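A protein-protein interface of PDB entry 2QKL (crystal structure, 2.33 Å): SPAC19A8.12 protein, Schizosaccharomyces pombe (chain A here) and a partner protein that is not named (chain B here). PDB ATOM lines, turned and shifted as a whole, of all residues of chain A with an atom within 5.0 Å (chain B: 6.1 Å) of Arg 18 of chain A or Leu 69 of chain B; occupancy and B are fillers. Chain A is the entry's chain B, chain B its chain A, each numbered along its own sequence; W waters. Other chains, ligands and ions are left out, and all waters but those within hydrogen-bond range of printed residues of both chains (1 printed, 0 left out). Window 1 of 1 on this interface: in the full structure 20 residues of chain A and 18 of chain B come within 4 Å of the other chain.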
ATOM      1  N   PHE A   3     -11.113  27.927   1.971  1.00  0.00           N
ATOM      2  CA  PHE A   3     -11.310  29.375   1.800  1.00  0.00           C
ATOM      3  C   PHE A   3     -12.655  29.840   2.355  1.00  0.00           C
ATOM      4  O   PHE A   3     -12.807  31.016   2.697  1.00  0.00           O
ATOM      5  CB  PHE A   3     -11.131  29.817   0.338  1.00  0.00           C
ATOM      6  CG  PHE A   3      -9.699  29.813  -0.124  1.00  0.00           C
ATOM      7  CD1 PHE A   3      -8.747  30.616   0.505  1.00  0.00           C
ATOM      8  CD2 PHE A   3      -9.303  29.004  -1.184  1.00  0.00           C
ATOM      9  CE1 PHE A   3      -7.421  30.616   0.077  1.00  0.00           C
ATOM     10  CE2 PHE A   3      -7.985  28.988  -1.617  1.00  0.00           C
ATOM     11  CZ  PHE A   3      -7.040  29.788  -0.988  1.00  0.00           C
ATOM     12  N   ASP A  13      -2.858  36.505   3.046  1.00  0.00           N
ATOM     13  CA  ASP A  13      -1.698  35.670   3.380  1.00  0.00           C
ATOM     14  C   ASP A  13      -1.486  34.594   2.321  1.00  0.00           C
ATOM     15  O   ASP A  13      -0.428  34.504   1.724  1.00  0.00           O
ATOM     16  CB  ASP A  13      -1.897  34.998   4.740  1.00  0.00           C
ATOM     17  CG  ASP A  13      -1.623  35.930   5.909  1.00  0.00           C
ATOM     18  OD1 ASP A  13      -0.970  36.983   5.729  1.00  0.00           O
ATOM     19  OD2 ASP A  13      -2.060  35.588   7.021  1.00  0.00           O
ATOM     20  N   ASP A  14      -2.516  33.786   2.091  1.00  0.00           N
ATOM     21  CA  ASP A  14      -2.499  32.768   1.058  1.00  0.00           C
ATOM     22  C   ASP A  14      -2.025  33.315  -0.286  1.00  0.00           C
ATOM     23  O   ASP A  14      -1.125  32.741  -0.906  1.00  0.00           O
ATOM     24  CB  ASP A  14      -3.878  32.118   0.922  1.00  0.00           C
ATOM     25  CG  ASP A  14      -3.893  31.003  -0.112  1.00  0.00           C
ATOM     26  OD1 ASP A  14      -3.706  29.831   0.282  1.00  0.00           O
ATOM     27  OD2 ASP A  14      -4.072  31.296  -1.318  1.00  0.00           O
ATOM     28  N   LEU A  15      -2.626  34.421  -0.727  1.00  0.00           N
ATOM     29  CA  LEU A  15      -2.319  35.006  -2.034  1.00  0.00           C
ATOM     30  C   LEU A  15      -0.876  35.522  -2.124  1.00  0.00           C
ATOM     31  O   LEU A  15      -0.248  35.414  -3.161  1.00  0.00           O
ATOM     32  CB  LEU A  15      -3.331  36.114  -2.386  1.00  0.00           C
ATOM     33  CG  LEU A  15      -4.792  35.699  -2.671  1.00  0.00           C
ATOM     34  CD1 LEU A  15      -5.697  36.919  -2.785  1.00  0.00           C
ATOM     35  CD2 LEU A  15      -4.952  34.812  -3.903  1.00  0.00           C
ATOM     36  N   SER A  16      -0.369  36.085  -1.033  1.00  0.00           N
ATOM     37  CA  SER A  16       1.019  36.506  -0.930  1.00  0.00           C
ATOM     38  C   SER A  16       1.982  35.329  -1.101  1.00  0.00           C
ATOM     39  O   SER A  16       2.930  35.409  -1.888  1.00  0.00           O
ATOM     40  CB  SER A  16       1.261  37.178   0.426  1.00  0.00           C
ATOM     41  OG  SER A  16       0.431  38.314   0.592  1.00  0.00           O
ATOM     42  N   ALA A  17       1.735  34.239  -0.370  1.00  0.00           N
ATOM     43  CA  ALA A  17       2.586  33.055  -0.439  1.00  0.00           C
ATOM     44  C   ALA A  17       2.464  32.307  -1.772  1.00  0.00           C
ATOM     45  O   ALA A  17       3.448  31.728  -2.248  1.00  0.00           O
ATOM     46  CB  ALA A  17       2.307  32.115   0.737  1.00  0.00           C
ATOM     47  N   ARG A  18       1.266  32.323  -2.361  1.00  0.00           N
ATOM     48  CA  ARG A  18       0.983  31.608  -3.609  1.00  0.00           C
ATOM     49  C   ARG A  18       1.496  32.350  -4.849  1.00  0.00           C
ATOM     50  O   ARG A  18       1.814  31.719  -5.866  1.00  0.00           O
ATOM     51  CB  ARG A  18      -0.536  31.346  -3.725  1.00  0.00           C
ATOM     52  CG  ARG A  18      -1.011  30.450  -4.878  1.00  0.00           C
ATOM     53  CD  ARG A  18      -2.542  30.310  -4.826  1.00  0.00           C
ATOM     54  NE  ARG A  18      -2.997  29.819  -3.524  1.00  0.00           N
ATOM     55  CZ  ARG A  18      -3.474  28.598  -3.288  1.00  0.00           C
ATOM     56  NH1 ARG A  18      -3.603  27.713  -4.268  1.00  0.00           N
ATOM     57  NH2 ARG A  18      -3.829  28.256  -2.053  1.00  0.00           N
ATOM     58  N   PHE A  19       1.575  33.679  -4.768  1.00  0.00           N
ATOM     59  CA  PHE A  19       1.902  34.501  -5.932  1.00  0.00           C
ATOM     60  C   PHE A  19       3.086  35.469  -5.794  1.00  0.00           C
ATOM     61  O   PHE A  19       3.780  35.723  -6.782  1.00  0.00           O
ATOM     62  CB  PHE A  19       0.661  35.281  -6.427  1.00  0.00           C
ATOM     63  CG  PHE A  19      -0.439  34.415  -6.997  1.00  0.00           C
ATOM     64  CD1 PHE A  19      -0.361  33.932  -8.299  1.00  0.00           C
ATOM     65  CD2 PHE A  19      -1.573  34.106  -6.234  1.00  0.00           C
ATOM     66  CE1 PHE A  19      -1.379  33.143  -8.831  1.00  0.00           C
ATOM     67  CE2 PHE A  19      -2.588  33.321  -6.755  1.00  0.00           C
ATOM     68  CZ  PHE A  19      -2.486  32.834  -8.064  1.00  0.00           C
ATOM     69  N   ILE A  20       3.326  36.004  -4.599  1.00  0.00           N
ATOM     70  CA  ILE A  20       4.239  37.158  -4.430  1.00  0.00           C
ATOM     71  C   ILE A  20       5.580  36.884  -3.711  1.00  0.00           C
ATOM     72  O   ILE A  20       6.641  37.313  -4.167  1.00  0.00           O
ATOM     73  CB  ILE A  20       3.518  38.346  -3.703  1.00  0.00           C
ATOM     74  CG1 ILE A  20       2.107  38.603  -4.282  1.00  0.00           C
ATOM     75  CG2 ILE A  20       4.403  39.608  -3.681  1.00  0.00           C
ATOM     76  CD1 ILE A  20       2.051  38.921  -5.794  1.00  0.00           C
ATOM     77  N   PHE A  44      -7.317  35.128  -9.287  1.00  0.00           N
ATOM     78  CA  PHE A  44      -7.501  33.989  -8.379  1.00  0.00           C
ATOM     79  C   PHE A  44      -8.496  34.318  -7.265  1.00  0.00           C
ATOM     80  O   PHE A  44      -9.366  33.506  -6.928  1.00  0.00           O
ATOM     81  CB  PHE A  44      -6.137  33.606  -7.768  1.00  0.00           C
ATOM     82  CG  PHE A  44      -6.094  32.231  -7.143  1.00  0.00           C
ATOM     83  CD1 PHE A  44      -5.637  31.135  -7.875  1.00  0.00           C
ATOM     84  CD2 PHE A  44      -6.473  32.039  -5.816  1.00  0.00           C
ATOM     85  CE1 PHE A  44      -5.581  29.867  -7.310  1.00  0.00           C
ATOM     86  CE2 PHE A  44      -6.431  30.766  -5.237  1.00  0.00           C
ATOM     87  CZ  PHE A  44      -5.981  29.676  -5.989  1.00  0.00           C
ATOM     88  N   ASN B  12       4.902  31.765   4.939  1.00  0.00           N
ATOM     89  CA  ASN B  12       4.761  30.518   4.153  1.00  0.00           C
ATOM     90  C   ASN B  12       4.182  29.350   4.969  1.00  0.00           C
ATOM     91  O   ASN B  12       3.234  28.698   4.531  1.00  0.00           O
ATOM     92  CB  ASN B  12       6.103  30.074   3.539  1.00  0.00           C
ATOM     93  CG  ASN B  12       6.514  30.895   2.320  1.00  0.00           C
ATOM     94  OD1 ASN B  12       7.711  31.069   2.059  1.00  0.00           O
ATOM     95  ND2 ASN B  12       5.543  31.372   1.558  1.00  0.00           N
ATOM     96  N   VAL B  15       0.469  29.694   6.054  1.00  0.00           N
ATOM     97  CA  VAL B  15      -0.416  29.389   4.915  1.00  0.00           C
ATOM     98  C   VAL B  15      -0.515  27.865   4.651  1.00  0.00           C
ATOM     99  O   VAL B  15      -1.605  27.328   4.422  1.00  0.00           O
ATOM    100  CB  VAL B  15       0.029  30.139   3.618  1.00  0.00           C
ATOM    101  CG1 VAL B  15      -0.809  29.713   2.421  1.00  0.00           C
ATOM    102  CG2 VAL B  15      -0.053  31.661   3.818  1.00  0.00           C
ATOM    103  N   LEU B  16       0.621  27.178   4.695  1.00  0.00           N
ATOM    104  CA  LEU B  16       0.639  25.734   4.530  1.00  0.00           C
ATOM    105  C   LEU B  16      -0.223  25.017   5.563  1.00  0.00           C
ATOM    106  O   LEU B  16      -0.981  24.128   5.216  1.00  0.00           O
ATOM    107  CB  LEU B  16       2.079  25.199   4.554  1.00  0.00           C
ATOM    108  CG  LEU B  16       2.940  25.626   3.361  1.00  0.00           C
ATOM    109  CD1 LEU B  16       4.383  25.161   3.537  1.00  0.00           C
ATOM    110  CD2 LEU B  16       2.362  25.102   2.057  1.00  0.00           C
ATOM    111  N   HIS B  19      -4.005  25.160   5.044  1.00  0.00           N
ATOM    112  CA  HIS B  19      -4.470  24.095   4.152  1.00  0.00           C
ATOM    113  C   HIS B  19      -4.255  22.686   4.725  1.00  0.00           C
ATOM    114  O   HIS B  19      -5.118  21.826   4.576  1.00  0.00           O
ATOM    115  CB  HIS B  19      -3.777  24.195   2.783  1.00  0.00           C
ATOM    116  CG  HIS B  19      -3.982  25.509   2.097  1.00  0.00           C
ATOM    117  ND1 HIS B  19      -5.137  25.821   1.420  1.00  0.00           N
ATOM    118  CD2 HIS B  19      -3.183  26.597   2.000  1.00  0.00           C
ATOM    119  CE1 HIS B  19      -5.043  27.041   0.928  1.00  0.00           C
ATOM    120  NE2 HIS B  19      -3.868  27.536   1.269  1.00  0.00           N
ATOM    121  N   TYR B  20      -3.099  22.461   5.357  1.00  0.00           N
ATOM    122  CA  TYR B  20      -2.716  21.147   5.898  1.00  0.00           C
ATOM    123  C   TYR B  20      -2.168  21.265   7.324  1.00  0.00           C
ATOM    124  O   TYR B  20      -0.966  21.460   7.506  1.00  0.00           O
ATOM    125  CB  TYR B  20      -1.668  20.485   5.005  1.00  0.00           C
ATOM    126  CG  TYR B  20      -2.001  20.506   3.528  1.00  0.00           C
ATOM    127  CD1 TYR B  20      -1.415  21.453   2.677  1.00  0.00           C
ATOM    128  CD2 TYR B  20      -2.906  19.588   2.985  1.00  0.00           C
ATOM    129  CE1 TYR B  20      -1.730  21.490   1.323  1.00  0.00           C
ATOM    130  CE2 TYR B  20      -3.226  19.612   1.634  1.00  0.00           C
ATOM    131  CZ  TYR B  20      -2.636  20.562   0.809  1.00  0.00           C
ATOM    132  OH  TYR B  20      -2.939  20.588  -0.526  1.00  0.00           O
ATOM    133  N   GLU B  51       0.423  23.756 -11.060  1.00  0.00           N
ATOM    134  CA  GLU B  51       1.646  24.526 -11.269  1.00  0.00           C
ATOM    135  C   GLU B  51       1.738  25.633 -10.222  1.00  0.00           C
ATOM    136  O   GLU B  51       0.769  26.352  -9.994  1.00  0.00           O
ATOM    137  CB  GLU B  51       1.616  25.135 -12.670  1.00  0.00           C
ATOM    138  CG  GLU B  51       2.951  25.501 -13.261  1.00  0.00           C
ATOM    139  CD  GLU B  51       2.783  26.320 -14.517  1.00  0.00           C
ATOM    140  OE1 GLU B  51       2.567  25.728 -15.596  1.00  0.00           O
ATOM    141  OE2 GLU B  51       2.854  27.565 -14.427  1.00  0.00           O
ATOM    142  N   GLY B  52       2.896  25.758  -9.580  1.00  0.00           N
ATOM    143  CA  GLY B  52       3.131  26.853  -8.651  1.00  0.00           C
ATOM    144  C   GLY B  52       4.400  26.679  -7.842  1.00  0.00           C
ATOM    145  O   GLY B  52       5.342  25.996  -8.264  1.00  0.00           O
ATOM    146  N   THR B  53       4.434  27.301  -6.672  1.00  0.00           N
ATOM    147  CA  THR B  53       5.566  27.146  -5.768  1.00  0.00           C
ATOM    148  C   THR B  53       5.519  25.777  -5.091  1.00  0.00           C
ATOM    149  O   THR B  53       4.462  25.321  -4.671  1.00  0.00           O
ATOM    150  CB  THR B  53       5.627  28.296  -4.727  1.00  0.00           C
ATOM    151  OG1 THR B  53       5.756  29.542  -5.420  1.00  0.00           O
ATOM    152  CG2 THR B  53       6.816  28.133  -3.785  1.00  0.00           C
ATOM    153  N   PHE B  54       6.691  25.164  -4.982  1.00  0.00           N
ATOM    154  CA  PHE B  54       6.911  23.844  -4.412  1.00  0.00           C
ATOM    155  C   PHE B  54       7.553  24.012  -3.028  1.00  0.00           C
ATOM    156  O   PHE B  54       8.621  24.597  -2.897  1.00  0.00           O
ATOM    157  CB  PHE B  54       7.833  23.087  -5.394  1.00  0.00           C
ATOM    158  CG  PHE B  54       8.425  21.792  -4.882  1.00  0.00           C
ATOM    159  CD1 PHE B  54       7.910  20.575  -5.291  1.00  0.00           C
ATOM    160  CD2 PHE B  54       9.564  21.789  -4.080  1.00  0.00           C
ATOM    161  CE1 PHE B  54       8.497  19.376  -4.865  1.00  0.00           C
ATOM    162  CE2 PHE B  54      10.138  20.604  -3.648  1.00  0.00           C
ATOM    163  CZ  PHE B  54       9.618  19.407  -4.041  1.00  0.00           C
ATOM    164  N   PHE B  55       6.879  23.500  -2.007  1.00  0.00           N
ATOM    165  CA  PHE B  55       7.389  23.480  -0.639  1.00  0.00           C
ATOM    166  C   PHE B  55       7.708  22.048  -0.210  1.00  0.00           C
ATOM    167  O   PHE B  55       6.815  21.220  -0.141  1.00  0.00           O
ATOM    168  CB  PHE B  55       6.353  24.061   0.328  1.00  0.00           C
ATOM    169  CG  PHE B  55       5.820  25.410  -0.080  1.00  0.00           C
ATOM    170  CD1 PHE B  55       6.293  26.571   0.519  1.00  0.00           C
ATOM    171  CD2 PHE B  55       4.826  25.521  -1.056  1.00  0.00           C
ATOM    172  CE1 PHE B  55       5.782  27.820   0.150  1.00  0.00           C
ATOM    173  CE2 PHE B  55       4.336  26.765  -1.440  1.00  0.00           C
ATOM    174  CZ  PHE B  55       4.812  27.916  -0.822  1.00  0.00           C
ATOM    175  N   VAL B  67       4.260  20.178  -0.952  1.00  0.00           N
ATOM    176  CA  VAL B  67       3.048  20.861  -1.362  1.00  0.00           C
ATOM    177  C   VAL B  67       3.392  21.804  -2.510  1.00  0.00           C
ATOM    178  O   VAL B  67       4.374  22.523  -2.446  1.00  0.00           O
ATOM    179  CB  VAL B  67       2.461  21.703  -0.187  1.00  0.00           C
ATOM    180  CG1 VAL B  67       1.277  22.571  -0.655  1.00  0.00           C
ATOM    181  CG2 VAL B  67       2.048  20.808   0.965  1.00  0.00           C
ATOM    182  N   ILE B  68       2.593  21.778  -3.570  1.00  0.00           N
ATOM    183  CA  ILE B  68       2.602  22.823  -4.578  1.00  0.00           C
ATOM    184  C   ILE B  68       1.314  23.623  -4.408  1.00  0.00           C
ATOM    185  O   ILE B  68       0.218  23.071  -4.520  1.00  0.00           O
ATOM    186  CB  ILE B  68       2.740  22.251  -6.012  1.00  0.00           C
ATOM    187  CG1 ILE B  68       4.079  21.510  -6.141  1.00  0.00           C
ATOM    188  CG2 ILE B  68       2.632  23.367  -7.078  1.00  0.00           C
ATOM    189  CD1 ILE B  68       4.240  20.703  -7.383  1.00  0.00           C
ATOM    190  N   LEU B  69       1.458  24.907  -4.088  1.00  0.00           N
ATOM    191  CA  LEU B  69       0.329  25.821  -3.997  1.00  0.00           C
ATOM    192  C   LEU B  69       0.007  26.276  -5.401  1.00  0.00           C
ATOM    193  O   LEU B  69       0.729  27.084  -5.981  1.00  0.00           O
ATOM    194  CB  LEU B  69       0.635  27.023  -3.091  1.00  0.00           C
ATOM    195  CG  LEU B  69       0.567  26.903  -1.555  1.00  0.00           C
ATOM    196  CD1 LEU B  69       0.613  28.309  -0.924  1.00  0.00           C
ATOM    197  CD2 LEU B  69      -0.659  26.135  -1.026  1.00  0.00           C
ATOM    198  N   ASN B  70      -1.087  25.737  -5.929  1.00  0.00           N
ATOM    199  CA  ASN B  70      -1.457  25.861  -7.326  1.00  0.00           C
ATOM    200  C   ASN B  70      -1.881  27.275  -7.696  1.00  0.00           C
ATOM    201  O   ASN B  70      -2.690  27.894  -7.002  1.00  0.00           O
ATOM    202  CB  ASN B  70      -2.579  24.854  -7.631  1.00  0.00           C
ATOM    203  CG  ASN B  70      -2.831  24.657  -9.123  1.00  0.00           C
ATOM    204  OD1 ASN B  70      -2.105  25.174  -9.970  1.00  0.00           O
ATOM    205  ND2 ASN B  70      -3.873  23.899  -9.444  1.00  0.00           N
ATOM    206  N   ARG B  71      -1.304  27.772  -8.788  1.00  0.00           N
ATOM    207  CA  ARG B  71      -1.642  29.077  -9.367  1.00  0.00           C
ATOM    208  C   ARG B  71      -2.833  29.037 -10.338  1.00  0.00           C
ATOM    209  O   ARG B  71      -3.462  30.068 -10.598  1.00  0.00           O
ATOM    210  CB  ARG B  71      -0.424  29.651 -10.096  1.00  0.00           C
ATOM    211  CG  ARG B  71       0.694  30.088  -9.169  1.00  0.00           C
ATOM    212  CD  ARG B  71       1.702  30.974  -9.867  1.00  0.00           C
ATOM    213  NE  ARG B  71       2.570  31.629  -8.889  1.00  0.00           N
ATOM    214  CZ  ARG B  71       3.815  31.261  -8.619  1.00  0.00           C
ATOM    215  NH1 ARG B  71       4.367  30.247  -9.275  1.00  0.00           N
ATOM    216  NH2 ARG B  71       4.519  31.921  -7.701  1.00  0.00           N
ATOM    217  N   SER B  73      -5.660  26.941 -10.143  1.00  0.00           N
ATOM    218  CA  SER B  73      -6.926  26.707  -9.452  1.00  0.00           C
ATOM    219  C   SER B  73      -6.641  26.558  -7.961  1.00  0.00           C
ATOM    220  O   SER B  73      -5.476  26.538  -7.565  1.00  0.00           O
ATOM    221  CB  SER B  73      -7.652  25.469 -10.016  1.00  0.00           C
ATOM    222  OG  SER B  73      -7.055  24.252  -9.599  1.00  0.00           O
ATOM    223  N   PRO B  74      -7.691  26.482  -7.115  1.00  0.00           N
ATOM    224  CA  PRO B  74      -7.414  26.252  -5.698  1.00  0.00           C
ATOM    225  C   PRO B  74      -7.043  24.805  -5.371  1.00  0.00           C
ATOM    226  O   PRO B  74      -6.773  24.500  -4.210  1.00  0.00           O
ATOM    227  CB  PRO B  74      -8.730  26.633  -5.003  1.00  0.00           C
ATOM    228  CG  PRO B  74      -9.630  27.159  -6.059  1.00  0.00           C
ATOM    229  CD  PRO B  74      -9.138  26.622  -7.358  1.00  0.00           C
ATOM    230  N   GLU B  75      -7.032  23.928  -6.379  1.00  0.00           N
ATOM    231  CA  GLU B  75      -6.574  22.541  -6.208  1.00  0.00           C
ATOM    232  C   GLU B  75      -5.059  22.438  -6.122  1.00  0.00           C
ATOM    233  O   GLU B  75      -4.366  22.629  -7.117  1.00  0.00           O
ATOM    234  CB  GLU B  75      -7.065  21.645  -7.342  1.00  0.00           C
ATOM    235  CG  GLU B  75      -8.207  20.720  -6.947  1.00  0.00           C
ATOM    236  CD  GLU B  75      -9.568  21.389  -7.030  1.00  0.00           C
ATOM    237  OE1 GLU B  75      -9.820  22.373  -6.292  1.00  0.00           O
ATOM    238  OE2 GLU B  75     -10.399  20.912  -7.834  1.00  0.00           O
ATOM    239  N   ASN B  76      -4.575  22.106  -4.929  1.00  0.00           N
ATOM    240  CA  ASN B  76      -3.157  21.957  -4.635  1.00  0.00           C
ATOM    241  C   ASN B  76      -2.746  20.504  -4.698  1.00  0.00           C
ATOM    242  O   ASN B  76      -3.595  19.622  -4.708  1.00  0.00           O
ATOM    243  CB  ASN B  76      -2.865  22.471  -3.226  1.00  0.00           C
ATOM    244  CG  ASN B  76      -3.361  23.878  -3.003  1.00  0.00           C
ATOM    245  OD1 ASN B  76      -3.259  24.740  -3.882  1.00  0.00           O
ATOM    246  ND2 ASN B  76      -3.890  24.127  -1.816  1.00  0.00           N
ATOM    247  N   LEU B  77      -1.442  20.258  -4.736  1.00  0.00           N
ATOM    248  CA  LEU B  77      -0.919  18.904  -4.637  1.00  0.00           C
ATOM    249  C   LEU B  77      -0.105  18.764  -3.351  1.00  0.00           C
ATOM    250  O   LEU B  77       0.711  19.625  -3.032  1.00  0.00           O
ATOM    251  CB  LEU B  77      -0.038  18.563  -5.848  1.00  0.00           C
ATOM    252  CG  LEU B  77       0.573  17.156  -5.966  1.00  0.00           C
ATOM    253  CD1 LEU B  77      -0.503  16.071  -5.845  1.00  0.00           C
ATOM    254  CD2 LEU B  77       1.319  17.008  -7.282  1.00  0.00           C
HETATM  255  O   HOH W   1       2.370  29.055  -5.487  1.00  0.00           O
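OD1 of Asp 14 of chain A lies within hydrogen-bond range of NE2 of His 19 of chain B, 2.5 Å away. NH1 of Arg 18 of chain A is in hydrogen-bond range of OD1 of Asn 76 of chain B (3.0 Å). NE2 of His 19 of chain B sits at hydrogen-bond distance from NH2 of Arg 18 of chain A (3.4 Å). O of Asn 70 of chain B is in hydrogen-bond range of NH1 of Arg 18 of chain A, 2.9 Å away. The guanidinium group of Arg 71 of chain B lies within hydrogen-bond range of the backbone carbonyl oxygen of Arg 18 of chain A (3.1 Å).
The backbone NH (N) of Arg 71 of chain B lies within hydrogen-bond range of the backbone carbonyl oxygen (O) of Glu 51 of chain B (2.8 Å). N of Leu 69 of chain B sits at hydrogen-bond distance from O of Thr 53 of chain B (3.1 Å). The backbone NH (N) of Glu 51 of chain B sits at hydrogen-bond distance from the side-chain amide oxygen (OD1) of Asn 70 of chain B (3.1 Å). OD1 of Asn 76 of chain B is in hydrogen-bond range of N of Asn 70 of chain B (3.1 Å). ND2 of Asn 70 of chain B lies within hydrogen-bond range of OG of Ser 73 of chain B, at 3.2 Å. OD1 of Asp 14 of chain A is in salt-bridge range of NH2 of Arg 18 of chain A.
CE1 of His 19 of chain B touches CZ of Phe 3 of chain A (3.9 Å). O of Asp 13 of chain A touches CG2 of Val 15 of chain B, 3.6 Å away. Asn 12 of chain B touches Ala 17 of chain A. Leu 69 of chain B touches Arg 18 of chain A (O to CG, 3.9 Å). O of Ser 73 of chain B touches NH1 of Arg 18 of chain A, 3.97 Å away. Phe 19 of chain A touches Arg 71 of chain B (CE1 to CG, 3.7 Å). CE1 of Phe 44 of chain A touches O of Asn 70 of chain B (3.5 Å). Arg 71 of chain B touches Phe 44 of chain A (O to CD1, 3.6 Å). Phe 44 of chain A touches Ser 73 of chain B. Pro 74 of chain B touches Phe 44 of chain A (CA to CZ, 3.7 Å).
Of chain A, only Arg 18 (3.9 Å) comes within 4 Å of Leu 69 of chain B. Of the printed residues of chain B, Ala 17 of chain A touches Asn 12 and Val 15. Of the printed residues of chain A, Pro 74 of chain B touches Phe 44. The nearest residue of chain B that does not touch Arg 18 of chain A is Pro 74 of chain B (4.3 Å).
Of the 20 printed residues of chain B, 9 touch a printed residue of chain A. Hydrophobic or aromatic side chains of chain B that line the printed part of chain A: Val 15, His 19 and Leu 69. Of the 10 printed residues of chain A, 7 touch a printed residue of chain B. Hydrophobic or aromatic side chains of chain A that line the printed part of chain B: Phe 3, Ala 17, Phe 19 and Phe 44. Among the printed residues, 17 pairs touch across the chains. Among the printed residues, no Asp or Glu carboxylate lies within 4 Å of a Lys or Arg side-chain nitrogen of the other chain.
Water W1 lies within hydrogen-bond range of O of Leu 69 of chain B (2.6 Å), O of Arg 18 of chain A (2.7 Å) and N of Thr 53 of chain B (3.0 Å).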
